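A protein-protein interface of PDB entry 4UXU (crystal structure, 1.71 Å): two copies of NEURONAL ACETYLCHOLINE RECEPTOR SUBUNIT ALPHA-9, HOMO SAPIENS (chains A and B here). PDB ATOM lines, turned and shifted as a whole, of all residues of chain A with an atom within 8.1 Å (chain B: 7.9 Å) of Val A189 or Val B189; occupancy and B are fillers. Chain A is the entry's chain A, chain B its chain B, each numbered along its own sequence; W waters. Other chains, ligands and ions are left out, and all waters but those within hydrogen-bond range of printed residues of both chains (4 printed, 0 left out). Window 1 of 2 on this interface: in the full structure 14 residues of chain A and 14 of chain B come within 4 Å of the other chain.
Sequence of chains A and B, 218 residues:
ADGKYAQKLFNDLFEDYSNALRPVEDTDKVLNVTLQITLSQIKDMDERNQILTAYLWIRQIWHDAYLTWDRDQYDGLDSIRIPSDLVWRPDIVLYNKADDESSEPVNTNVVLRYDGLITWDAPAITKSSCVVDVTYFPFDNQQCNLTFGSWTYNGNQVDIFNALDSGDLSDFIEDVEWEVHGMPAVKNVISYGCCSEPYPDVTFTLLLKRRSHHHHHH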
ATOM      1  N   ASN A 154      18.433  40.223   9.627  1.00  0.00           N
ATOM      2  CA  ASN A 154      17.805  39.130   8.866  1.00  0.00           C
ATOM      3  C   ASN A 154      18.438  37.796   9.231  1.00  0.00           C
ATOM      4  O   ASN A 154      19.399  37.759   9.979  1.00  0.00           O
ATOM      5  CB  ASN A 154      17.882  39.354   7.346  1.00  0.00           C
ATOM      6  CG  ASN A 154      19.301  39.373   6.811  1.00  0.00           C
ATOM      7  OD1 ASN A 154      20.065  38.415   6.972  1.00  0.00           O
ATOM      8  ND2 ASN A 154      19.645  40.459   6.117  1.00  0.00           N
ATOM      9  N   GLY A 155      17.932  36.714   8.648  1.00  0.00           N
ATOM     10  CA  GLY A 155      18.371  35.371   9.001  1.00  0.00           C
ATOM     11  C   GLY A 155      19.777  34.999   8.571  1.00  0.00           C
ATOM     12  O   GLY A 155      20.331  34.015   9.053  1.00  0.00           O
ATOM     13  N   ASN A 156      20.366  35.760   7.656  1.00  0.00           N
ATOM     14  CA  ASN A 156      21.764  35.525   7.293  1.00  0.00           C
ATOM     15  C   ASN A 156      22.743  36.256   8.208  1.00  0.00           C
ATOM     16  O   ASN A 156      23.957  36.051   8.125  1.00  0.00           O
ATOM     17  CB  ASN A 156      22.016  35.916   5.835  1.00  0.00           C
ATOM     18  CG  ASN A 156      21.405  34.932   4.868  1.00  0.00           C
ATOM     19  OD1 ASN A 156      21.462  33.726   5.084  1.00  0.00           O
ATOM     20  ND2 ASN A 156      20.797  35.442   3.809  1.00  0.00           N
ATOM     21  N   ASP A 159      20.705  34.102  13.078  1.00  0.00           N
ATOM     22  CA  ASP A 159      19.777  33.008  12.867  1.00  0.00           C
ATOM     23  C   ASP A 159      19.397  32.452  14.236  1.00  0.00           C
ATOM     24  O   ASP A 159      20.265  32.235  15.066  1.00  0.00           O
ATOM     25  CB  ASP A 159      20.416  31.943  11.979  1.00  0.00           C
ATOM     26  CG  ASP A 159      19.410  30.964  11.401  1.00  0.00           C
ATOM     27  OD1 ASP A 159      18.180  31.165  11.572  1.00  0.00           O
ATOM     28  OD2 ASP A 159      19.873  29.997  10.757  1.00  0.00           O
ATOM     29  N   ILE A 160      18.099  32.275  14.463  1.00  0.00           N
ATOM     30  CA  ILE A 160      17.552  31.912  15.771  1.00  0.00           C
ATOM     31  C   ILE A 160      17.126  30.432  15.758  1.00  0.00           C
ATOM     32  O   ILE A 160      16.716  29.906  14.726  1.00  0.00           O
ATOM     33  CB  ILE A 160      16.367  32.838  16.123  1.00  0.00           C
ATOM     34  CG1 ILE A 160      15.843  32.630  17.538  1.00  0.00           C
ATOM     35  CG2 ILE A 160      15.234  32.731  15.104  1.00  0.00           C
ATOM     36  CD1 ILE A 160      14.790  33.684  17.884  1.00  0.00           C
ATOM     37  N   VAL A 186       7.995  26.072  17.410  1.00  0.00           N
ATOM     38  CA  VAL A 186       8.421  25.833  16.030  1.00  0.00           C
ATOM     39  C   VAL A 186       9.337  26.960  15.586  1.00  0.00           C
ATOM     40  O   VAL A 186       9.388  28.008  16.220  1.00  0.00           O
ATOM     41  CB  VAL A 186       7.240  25.737  15.035  1.00  0.00           C
ATOM     42  CG1 VAL A 186       6.271  24.619  15.427  1.00  0.00           C
ATOM     43  CG2 VAL A 186       6.529  27.080  14.911  1.00  0.00           C
ATOM     44  N   LYS A 187      10.065  26.739  14.499  1.00  0.00           N
ATOM     45  CA  LYS A 187      10.834  27.801  13.872  1.00  0.00           C
ATOM     46  C   LYS A 187      10.287  28.034  12.470  1.00  0.00           C
ATOM     47  O   LYS A 187      10.167  27.090  11.691  1.00  0.00           O
ATOM     48  CB  LYS A 187      12.320  27.447  13.809  1.00  0.00           C
ATOM     49  CG  LYS A 187      13.138  28.438  12.979  1.00  0.00           C
ATOM     50  CD  LYS A 187      14.604  28.004  12.907  1.00  0.00           C
ATOM     51  CE  LYS A 187      15.434  28.984  12.100  1.00  0.00           C
ATOM     52  NZ  LYS A 187      16.907  28.724  12.223  1.00  0.00           N
ATOM     53  N   ASN A 188       9.939  29.282  12.173  1.00  0.00           N
ATOM     54  CA  ASN A 188       9.458  29.656  10.846  1.00  0.00           C
ATOM     55  C   ASN A 188      10.487  30.510  10.136  1.00  0.00           C
ATOM     56  O   ASN A 188      11.117  31.356  10.767  1.00  0.00           O
ATOM     57  CB  ASN A 188       8.142  30.442  10.927  1.00  0.00           C
ATOM     58  CG  ASN A 188       7.029  29.664  11.577  1.00  0.00           C
ATOM     59  OD1 ASN A 188       6.468  28.735  10.985  1.00  0.00           O
ATOM     60  ND2 ASN A 188       6.665  30.067  12.788  1.00  0.00           N
ATOM     61  N   VAL A 189      10.644  30.317   8.826  1.00  0.00           N
ATOM     62  CA  VAL A 189      11.455  31.240   8.048  1.00  0.00           C
ATOM     63  C   VAL A 189      10.667  31.617   6.812  1.00  0.00           C
ATOM     64  O   VAL A 189      10.136  30.747   6.116  1.00  0.00           O
ATOM     65  CB  VAL A 189      12.809  30.646   7.610  1.00  0.00           C
ATOM     66  CG1 VAL A 189      13.685  31.735   6.989  1.00  0.00           C
ATOM     67  CG2 VAL A 189      13.519  29.967   8.765  1.00  0.00           C
ATOM     68  N   ILE A 190      10.585  32.908   6.533  1.00  0.00           N
ATOM     69  CA  ILE A 190       9.945  33.342   5.305  1.00  0.00           C
ATOM     70  C   ILE A 190      10.872  34.215   4.473  1.00  0.00           C
ATOM     71  O   ILE A 190      11.658  35.004   5.003  1.00  0.00           O
ATOM     72  CB  ILE A 190       8.625  34.093   5.598  1.00  0.00           C
ATOM     73  CG1 ILE A 190       7.838  34.333   4.309  1.00  0.00           C
ATOM     74  CG2 ILE A 190       8.885  35.412   6.326  1.00  0.00           C
ATOM     75  CD1 ILE A 190       6.417  34.807   4.553  1.00  0.00           C
ATOM     76  N   SER A 191      10.795  34.047   3.157  1.00  0.00           N
ATOM     77  CA  SER A 191      11.459  34.963   2.251  1.00  0.00           C
ATOM     78  C   SER A 191      10.498  35.279   1.125  1.00  0.00           C
ATOM     79  O   SER A 191       9.690  34.436   0.726  1.00  0.00           O
ATOM     80  CB  SER A 191      12.773  34.377   1.729  1.00  0.00           C
ATOM     81  OG  SER A 191      12.579  33.141   1.082  1.00  0.00           O
ATOM     82  N   TYR A 192      10.582  36.510   0.637  1.00  0.00           N
ATOM     83  CA  TYR A 192       9.653  37.041  -0.360  1.00  0.00           C
ATOM     84  C   TYR A 192      10.248  37.034  -1.766  1.00  0.00           C
ATOM     85  O   TYR A 192      11.387  37.454  -1.969  1.00  0.00           O
ATOM     86  CB  TYR A 192       9.241  38.467   0.030  1.00  0.00           C
ATOM     87  CG  TYR A 192       8.407  38.493   1.289  1.00  0.00           C
ATOM     88  CD1 TYR A 192       9.003  38.479   2.541  1.00  0.00           C
ATOM     89  CD2 TYR A 192       7.017  38.488   1.219  1.00  0.00           C
ATOM     90  CE1 TYR A 192       8.239  38.474   3.694  1.00  0.00           C
ATOM     91  CE2 TYR A 192       6.247  38.491   2.358  1.00  0.00           C
ATOM     92  CZ  TYR A 192       6.862  38.479   3.593  1.00  0.00           C
ATOM     93  OH  TYR A 192       6.096  38.479   4.731  1.00  0.00           O
ATOM     94  N   GLU A 197      16.114  38.585   1.441  1.00  0.00           N
ATOM     95  CA  GLU A 197      16.710  37.967   2.612  1.00  0.00           C
ATOM     96  C   GLU A 197      15.674  37.122   3.362  1.00  0.00           C
ATOM     97  O   GLU A 197      14.471  37.314   3.208  1.00  0.00           O
ATOM     98  CB  GLU A 197      17.297  39.048   3.518  1.00  0.00           C
ATOM     99  CG  GLU A 197      18.465  39.810   2.889  1.00  0.00           C
ATOM    100  CD  GLU A 197      19.635  38.900   2.527  1.00  0.00           C
ATOM    101  OE1 GLU A 197      20.259  38.323   3.443  1.00  0.00           O
ATOM    102  OE2 GLU A 197      19.928  38.753   1.321  1.00  0.00           O
ATOM    103  N   PRO A 198      16.143  36.172   4.182  1.00  0.00           N
ATOM    104  CA  PRO A 198      15.248  35.347   5.003  1.00  0.00           C
ATOM    105  C   PRO A 198      14.929  36.000   6.359  1.00  0.00           C
ATOM    106  O   PRO A 198      15.792  36.628   6.962  1.00  0.00           O
ATOM    107  CB  PRO A 198      16.055  34.067   5.199  1.00  0.00           C
ATOM    108  CG  PRO A 198      17.485  34.585   5.282  1.00  0.00           C
ATOM    109  CD  PRO A 198      17.543  35.713   4.265  1.00  0.00           C
ATOM    110  N   TYR A 199      13.690  35.858   6.813  1.00  0.00           N
ATOM    111  CA  TYR A 199      13.274  36.409   8.093  1.00  0.00           C
ATOM    112  C   TYR A 199      12.762  35.279   8.995  1.00  0.00           C
ATOM    113  O   TYR A 199      11.643  34.790   8.831  1.00  0.00           O
ATOM    114  CB  TYR A 199      12.203  37.484   7.895  1.00  0.00           C
ATOM    115  CG  TYR A 199      12.605  38.561   6.915  1.00  0.00           C
ATOM    116  CD1 TYR A 199      13.621  39.462   7.221  1.00  0.00           C
ATOM    117  CD2 TYR A 199      11.970  38.680   5.689  1.00  0.00           C
ATOM    118  CE1 TYR A 199      13.997  40.450   6.318  1.00  0.00           C
ATOM    119  CE2 TYR A 199      12.335  39.667   4.788  1.00  0.00           C
ATOM    120  CZ  TYR A 199      13.349  40.544   5.107  1.00  0.00           C
ATOM    121  OH  TYR A 199      13.713  41.523   4.211  1.00  0.00           O
ATOM    122  N   PRO A 200      13.597  34.852   9.948  1.00  0.00           N
ATOM    123  CA  PRO A 200      13.234  33.727  10.813  1.00  0.00           C
ATOM    124  C   PRO A 200      12.521  34.186  12.072  1.00  0.00           C
ATOM    125  O   PRO A 200      12.709  35.323  12.514  1.00  0.00           O
ATOM    126  CB  PRO A 200      14.584  33.110  11.137  1.00  0.00           C
ATOM    127  CG  PRO A 200      15.494  34.287  11.202  1.00  0.00           C
ATOM    128  CD  PRO A 200      15.008  35.238  10.120  1.00  0.00           C
ATOM    129  N   ASP A 201      11.701  33.317  12.644  1.00  0.00           N
ATOM    130  CA  ASP A 201      11.174  33.553  13.985  1.00  0.00           C
ATOM    131  C   ASP A 201      11.088  32.218  14.687  1.00  0.00           C
ATOM    132  O   ASP A 201      11.160  31.179  14.046  1.00  0.00           O
ATOM    133  CB  ASP A 201       9.786  34.208  13.958  1.00  0.00           C
ATOM    134  CG  ASP A 201       8.701  33.279  13.397  1.00  0.00           C
ATOM    135  OD1 ASP A 201       8.346  32.262  14.055  1.00  0.00           O
ATOM    136  OD2 ASP A 201       8.180  33.561  12.296  1.00  0.00           O
ATOM    137  N   VAL A 202      10.922  32.255  16.003  1.00  0.00           N
ATOM    138  CA  VAL A 202      10.477  31.060  16.710  1.00  0.00           C
ATOM    139  C   VAL A 202       9.141  31.403  17.328  1.00  0.00           C
ATOM    140  O   VAL A 202       8.947  32.511  17.849  1.00  0.00           O
ATOM    141  CB  VAL A 202      11.483  30.563  17.775  1.00  0.00           C
ATOM    142  CG1 VAL A 202      12.786  30.136  17.116  1.00  0.00           C
ATOM    143  CG2 VAL A 202      11.723  31.614  18.851  1.00  0.00           C
ATOM    144  N   GLY B 155      14.307  19.725   3.670  1.00  0.00           N
ATOM    145  CA  GLY B 155      14.985  20.896   3.128  1.00  0.00           C
ATOM    146  C   GLY B 155      16.495  20.787   3.087  1.00  0.00           C
ATOM    147  O   GLY B 155      17.156  21.572   2.418  1.00  0.00           O
ATOM    148  N   ASN B 156      17.052  19.820   3.807  1.00  0.00           N
ATOM    149  CA  ASN B 156      18.486  19.571   3.724  1.00  0.00           C
ATOM    150  C   ASN B 156      18.840  18.593   2.598  1.00  0.00           C
ATOM    151  O   ASN B 156      20.018  18.356   2.311  1.00  0.00           O
ATOM    152  CB  ASN B 156      19.004  19.055   5.062  1.00  0.00           C
ATOM    153  CG  ASN B 156      19.072  20.146   6.105  1.00  0.00           C
ATOM    154  OD1 ASN B 156      19.307  21.308   5.783  1.00  0.00           O
ATOM    155  ND2 ASN B 156      18.851  19.785   7.354  1.00  0.00           N
ATOM    156  N   ASP B 159      16.197  21.553  -1.479  1.00  0.00           N
ATOM    157  CA  ASP B 159      15.809  22.889  -1.065  1.00  0.00           C
ATOM    158  C   ASP B 159      15.203  23.591  -2.278  1.00  0.00           C
ATOM    159  O   ASP B 159      15.734  23.508  -3.379  1.00  0.00           O
ATOM    160  CB  ASP B 159      17.010  23.644  -0.507  1.00  0.00           C
ATOM    161  CG  ASP B 159      16.616  24.854   0.310  1.00  0.00           C
ATOM    162  OD1 ASP B 159      15.401  25.072   0.549  1.00  0.00           O
ATOM    163  OD2 ASP B 159      17.537  25.583   0.730  1.00  0.00           O
ATOM    164  N   ILE B 160      14.069  24.249  -2.070  1.00  0.00           N
ATOM    165  CA  ILE B 160      13.272  24.783  -3.168  1.00  0.00           C
ATOM    166  C   ILE B 160      13.299  26.309  -3.124  1.00  0.00           C
ATOM    167  O   ILE B 160      13.297  26.895  -2.053  1.00  0.00           O
ATOM    168  CB  ILE B 160      11.835  24.261  -3.078  1.00  0.00           C
ATOM    169  CG1 ILE B 160      10.981  24.701  -4.258  1.00  0.00           C
ATOM    170  CG2 ILE B 160      11.174  24.657  -1.761  1.00  0.00           C
ATOM    171  CD1 ILE B 160       9.579  24.107  -4.182  1.00  0.00           C
ATOM    172  N   VAL B 186       5.978  33.434  -2.065  1.00  0.00           N
ATOM    173  CA  VAL B 186       6.884  33.431  -0.922  1.00  0.00           C
ATOM    174  C   VAL B 186       7.494  32.051  -0.732  1.00  0.00           C
ATOM    175  O   VAL B 186       7.077  31.085  -1.360  1.00  0.00           O
ATOM    176  CB  VAL B 186       6.181  33.843   0.398  1.00  0.00           C
ATOM    177  CG1 VAL B 186       5.559  35.223   0.259  1.00  0.00           C
ATOM    178  CG2 VAL B 186       5.140  32.794   0.818  1.00  0.00           C
ATOM    179  N   LYS B 187       8.521  31.974   0.104  1.00  0.00           N
ATOM    180  CA  LYS B 187       9.072  30.687   0.499  1.00  0.00           C
ATOM    181  C   LYS B 187       8.937  30.547   2.008  1.00  0.00           C
ATOM    182  O   LYS B 187       9.362  31.433   2.750  1.00  0.00           O
ATOM    183  CB  LYS B 187      10.541  30.543   0.081  1.00  0.00           C
ATOM    184  CG  LYS B 187      11.243  29.317   0.698  1.00  0.00           C
ATOM    185  CD  LYS B 187      12.708  29.218   0.247  1.00  0.00           C
ATOM    186  CE  LYS B 187      13.373  27.969   0.815  1.00  0.00           C
ATOM    187  NZ  LYS B 187      14.788  27.811   0.339  1.00  0.00           N
ATOM    188  N   ASN B 188       8.351  29.441   2.449  1.00  0.00           N
ATOM    189  CA  ASN B 188       8.242  29.169   3.885  1.00  0.00           C
ATOM    190  C   ASN B 188       9.100  27.986   4.268  1.00  0.00           C
ATOM    191  O   ASN B 188       9.190  27.018   3.524  1.00  0.00           O
ATOM    192  CB  ASN B 188       6.797  28.879   4.292  1.00  0.00           C
ATOM    193  CG  ASN B 188       5.855  30.003   3.951  1.00  0.00           C
ATOM    194  OD1 ASN B 188       5.842  31.053   4.615  1.00  0.00           O
ATOM    195  ND2 ASN B 188       5.027  29.783   2.929  1.00  0.00           N
ATOM    196  N   VAL B 189       9.723  28.052   5.438  1.00  0.00           N
ATOM    197  CA  VAL B 189      10.399  26.886   5.970  1.00  0.00           C
ATOM    198  C   VAL B 189       9.968  26.739   7.416  1.00  0.00           C
ATOM    199  O   VAL B 189       9.980  27.703   8.176  1.00  0.00           O
ATOM    200  CB  VAL B 189      11.939  26.991   5.901  1.00  0.00           C
ATOM    201  CG1 VAL B 189      12.578  25.643   6.299  1.00  0.00           C
ATOM    202  CG2 VAL B 189      12.401  27.438   4.528  1.00  0.00           C
ATOM    203  N   ILE B 190       9.563  25.537   7.795  1.00  0.00           N
ATOM    204  CA  ILE B 190       9.222  25.291   9.185  1.00  0.00           C
ATOM    205  C   ILE B 190      10.044  24.132   9.726  1.00  0.00           C
ATOM    206  O   ILE B 190      10.332  23.177   9.017  1.00  0.00           O
ATOM    207  CB  ILE B 190       7.709  25.006   9.356  1.00  0.00           C
ATOM    208  CG1 ILE B 190       7.325  24.934  10.831  1.00  0.00           C
ATOM    209  CG2 ILE B 190       7.300  23.713   8.665  1.00  0.00           C
ATOM    210  CD1 ILE B 190       5.838  24.930  11.046  1.00  0.00           C
ATOM    211  N   SER B 191      10.447  24.233  10.984  1.00  0.00           N
ATOM    212  CA  SER B 191      11.077  23.120  11.659  1.00  0.00           C
ATOM    213  C   SER B 191      10.477  23.055  13.040  1.00  0.00           C
ATOM    214  O   SER B 191      10.149  24.088  13.628  1.00  0.00           O
ATOM    215  CB  SER B 191      12.598  23.274  11.705  1.00  0.00           C
ATOM    216  OG  SER B 191      12.966  24.485  12.320  1.00  0.00           O
ATOM    217  N   TYR B 192      10.328  21.841  13.550  1.00  0.00           N
ATOM    218  CA  TYR B 192       9.620  21.603  14.805  1.00  0.00           C
ATOM    219  C   TYR B 192      10.557  21.331  15.962  1.00  0.00           C
ATOM    220  O   TYR B 192      11.469  20.512  15.855  1.00  0.00           O
ATOM    221  CB  TYR B 192       8.664  20.421  14.646  1.00  0.00           C
ATOM    222  CG  TYR B 192       7.504  20.724  13.738  1.00  0.00           C
ATOM    223  CD1 TYR B 192       7.611  20.564  12.358  1.00  0.00           C
ATOM    224  CD2 TYR B 192       6.304  21.187  14.255  1.00  0.00           C
ATOM    225  CE1 TYR B 192       6.548  20.855  11.522  1.00  0.00           C
ATOM    226  CE2 TYR B 192       5.230  21.472  13.424  1.00  0.00           C
ATOM    227  CZ  TYR B 192       5.361  21.304  12.064  1.00  0.00           C
ATOM    228  OH  TYR B 192       4.293  21.595  11.242  1.00  0.00           O
ATOM    229  N   GLU B 197      14.248  18.159  11.188  1.00  0.00           N
ATOM    230  CA  GLU B 197      14.641  18.557   9.841  1.00  0.00           C
ATOM    231  C   GLU B 197      13.779  19.736   9.393  1.00  0.00           C
ATOM    232  O   GLU B 197      12.666  19.901   9.885  1.00  0.00           O
ATOM    233  CB  GLU B 197      14.480  17.373   8.883  1.00  0.00           C
ATOM    234  CG  GLU B 197      15.165  16.091   9.331  1.00  0.00           C
ATOM    235  CD  GLU B 197      14.500  15.429  10.548  1.00  0.00           C
ATOM    236  OE1 GLU B 197      13.304  15.696  10.821  1.00  0.00           O
ATOM    237  OE2 GLU B 197      15.187  14.658  11.250  1.00  0.00           O
ATOM    238  N   PRO B 198      14.284  20.554   8.448  1.00  0.00           N
ATOM    239  CA  PRO B 198      13.516  21.675   7.891  1.00  0.00           C
ATOM    240  C   PRO B 198      12.578  21.232   6.765  1.00  0.00           C
ATOM    241  O   PRO B 198      12.962  20.371   5.969  1.00  0.00           O
ATOM    242  CB  PRO B 198      14.607  22.609   7.369  1.00  0.00           C
ATOM    243  CG  PRO B 198      15.722  21.679   6.977  1.00  0.00           C
ATOM    244  CD  PRO B 198      15.673  20.533   7.950  1.00  0.00           C
ATOM    245  N   TYR B 199      11.366  21.786   6.722  1.00  0.00           N
ATOM    246  CA  TYR B 199      10.408  21.475   5.660  1.00  0.00           C
ATOM    247  C   TYR B 199       9.997  22.738   4.901  1.00  0.00           C
ATOM    248  O   TYR B 199       9.171  23.516   5.375  1.00  0.00           O
ATOM    249  CB  TYR B 199       9.164  20.793   6.229  1.00  0.00           C
ATOM    250  CG  TYR B 199       9.486  19.598   7.090  1.00  0.00           C
ATOM    251  CD1 TYR B 199       9.965  18.416   6.534  1.00  0.00           C
ATOM    252  CD2 TYR B 199       9.328  19.658   8.462  1.00  0.00           C
ATOM    253  CE1 TYR B 199      10.272  17.326   7.334  1.00  0.00           C
ATOM    254  CE2 TYR B 199       9.623  18.584   9.258  1.00  0.00           C
ATOM    255  CZ  TYR B 199      10.097  17.422   8.698  1.00  0.00           C
ATOM    256  OH  TYR B 199      10.394  16.363   9.516  1.00  0.00           O
ATOM    257  N   PRO B 200      10.583  22.943   3.718  1.00  0.00           N
ATOM    258  CA  PRO B 200      10.318  24.160   2.936  1.00  0.00           C
ATOM    259  C   PRO B 200       9.140  24.014   1.981  1.00  0.00           C
ATOM    260  O   PRO B 200       8.851  22.905   1.522  1.00  0.00           O
ATOM    261  CB  PRO B 200      11.607  24.335   2.144  1.00  0.00           C
ATOM    262  CG  PRO B 200      12.027  22.924   1.869  1.00  0.00           C
ATOM    263  CD  PRO B 200      11.705  22.172   3.160  1.00  0.00           C
ATOM    264  N   ASP B 201       8.489  25.129   1.661  1.00  0.00           N
ATOM    265  CA  ASP B 201       7.550  25.166   0.544  1.00  0.00           C
ATOM    266  C   ASP B 201       7.688  26.496  -0.178  1.00  0.00           C
ATOM    267  O   ASP B 201       8.289  27.426   0.354  1.00  0.00           O
ATOM    268  CB  ASP B 201       6.100  24.983   1.012  1.00  0.00           C
ATOM    269  CG  ASP B 201       5.580  26.172   1.832  1.00  0.00           C
ATOM    270  OD1 ASP B 201       5.379  27.278   1.262  1.00  0.00           O
ATOM    271  OD2 ASP B 201       5.347  26.006   3.049  1.00  0.00           O
ATOM    272  N   VAL B 202       7.137  26.576  -1.384  1.00  0.00           N
ATOM    273  CA  VAL B 202       6.860  27.879  -1.978  1.00  0.00           C
ATOM    274  C   VAL B 202       5.355  27.984  -2.109  1.00  0.00           C
ATOM    275  O   VAL B 202       4.676  27.014  -2.464  1.00  0.00           O
ATOM    276  CB  VAL B 202       7.559  28.083  -3.335  1.00  0.00           C
ATOM    277  CG1 VAL B 202       9.064  28.001  -3.159  1.00  0.00           C
ATOM    278  CG2 VAL B 202       7.080  27.065  -4.374  1.00  0.00           C
HETATM  279  O   HOH W   1      12.145  31.268   3.452  1.00  0.00           O
HETATM  280  O   HOH W   2       6.843  28.479   8.297  1.00  0.00           O
HETATM  281  O   HOH W   3      12.618  26.363   9.946  1.00  0.00           O
HETATM  282  O   HOH W   4       7.044  31.033   7.017  1.00  0.00           O
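OD1 of Asp A159 is in salt-bridge range of NZ of Lys A187, 2.8 Å away.
O of Asn A188 lies within hydrogen-bond range of N of Asp A201 (2.8 Å).
O of Ile A190 sits at hydrogen-bond distance from N of Tyr A199 (2.9 Å).
The side-chain amino group (NZ) of Lys B187 is in salt-bridge range of the side-chain carboxylate (OD1) of Asp B159.
O of Ile B160 is in hydrogen-bond range of NZ of Lys B187 (3.0 Å).
The backbone NH (N) of Asp B201 lies within hydrogen-bond range of the backbone carbonyl oxygen (O) of Asn B188 (2.7 Å).
Water W4 bridges OD1 of Asn B188 and O of Val A189.
Water W2 bridges OD1 of Asn A188 (2.7 Å) and O of Val B189 (3.2 Å).
Water W1 lies within hydrogen-bond range of O of Lys B187 (2.9 Å), OG of Ser A191 (3.1 Å) and O of Val A189 (3.4 Å).
Water W3 lies within hydrogen-bond range of OG of Ser B191 (3.0 Å), O of Lys A187 (3.1 Å) and O of Val B189 (3.4 Å).
Val A189 touches just these residues of chain B: Lys B187, Asn B188 and Val B189.
Printed residues of chain A within 4 Å of Val B189: Lys A187, Asn A188 and Val A189.
Printed residues of chain B within 4 Å of Tyr A192: Val B186.
Printed residues of chain A within 4 Å of Tyr B192: Val A186 (3.6 Å).
Printed residues of chain B within 4 Å of Val A186: Ser B191 (3.4 Å) and Tyr B192 (3.6 Å).
Of the printed residues of chain A, Ser B191 touches Val A186 and Lys A187.
Of the printed residues of chain A, Val B186 touches Ser A191 (3.4 Å) and Tyr A192 (3.7 Å).
Asn A156 touches none of the printed residues of chain B.
Among the printed residues, merely in contact across the chains: Val A186 with Ser B191 (3.4 Å), Val A186 with Tyr B192 (3.6 Å), Lys A187 with Val B189 (3.6 Å), Lys A187 with Ile B190 (3.2 Å), Asn A188 with Val B189 (3.3 Å), Asn A188 with Ile B190 (3.9 Å), Val A189 with Lys B187 (3.5 Å), Val A189 with Asn B188 (3.3 Å), Ile A190 with Lys B187 (3.2 Å), Ile A190 with Asn B188 (3.8 Å), Ser A191 with Val B186 (3.4 Å) and Tyr A192 with Val B186 (3.7 Å).
Of the 17 printed residues of chain B, 7 touch a printed residue of chain A.
Hydrophobic or aromatic side chains of chain B that line the printed part of chain A: Val B186, Ile B190 and Tyr B192.
Printed residues of chain A that touch a printed residue of chain B: Val A186, Lys A187, Asn A188, Val A189, Ile A190, Ser A191 and Tyr A192.
Hydrophobic or aromatic side chains of chain A that line the printed part of chain B: Val A186, Ile A190 and Tyr A192.
Among the printed residues, 15 pairs touch across the chains.
The backbone NH of Lys A187 is in hydrogen-bond range of the backbone carbonyl oxygen of Ser B191 (2.8 Å).
The backbone NH of Val A189 sits at hydrogen-bond distance from the backbone carbonyl oxygen of Val B189 (2.8 Å).
The backbone NH (N) of Lys B187 sits at hydrogen-bond distance from the backbone carbonyl oxygen (O) of Ser A191 (2.8 Å).
Val A186 touches Tyr B192, and with the chains exchanged Tyr A192 touches Val B186.
Lys A187 touches Val B189, and with the chains exchanged Val A189 touches Lys B187.
Lys A187 touches Ile B190, and with the chains exchanged Ile A190 touches Lys B187.
Asn A188 touches Val B189, and with the chains exchanged Val A189 touches Asn B188.
Of the 15 pairs that touch across the chains among the printed residues, 15 have their exchanged pair printed and touching as well.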
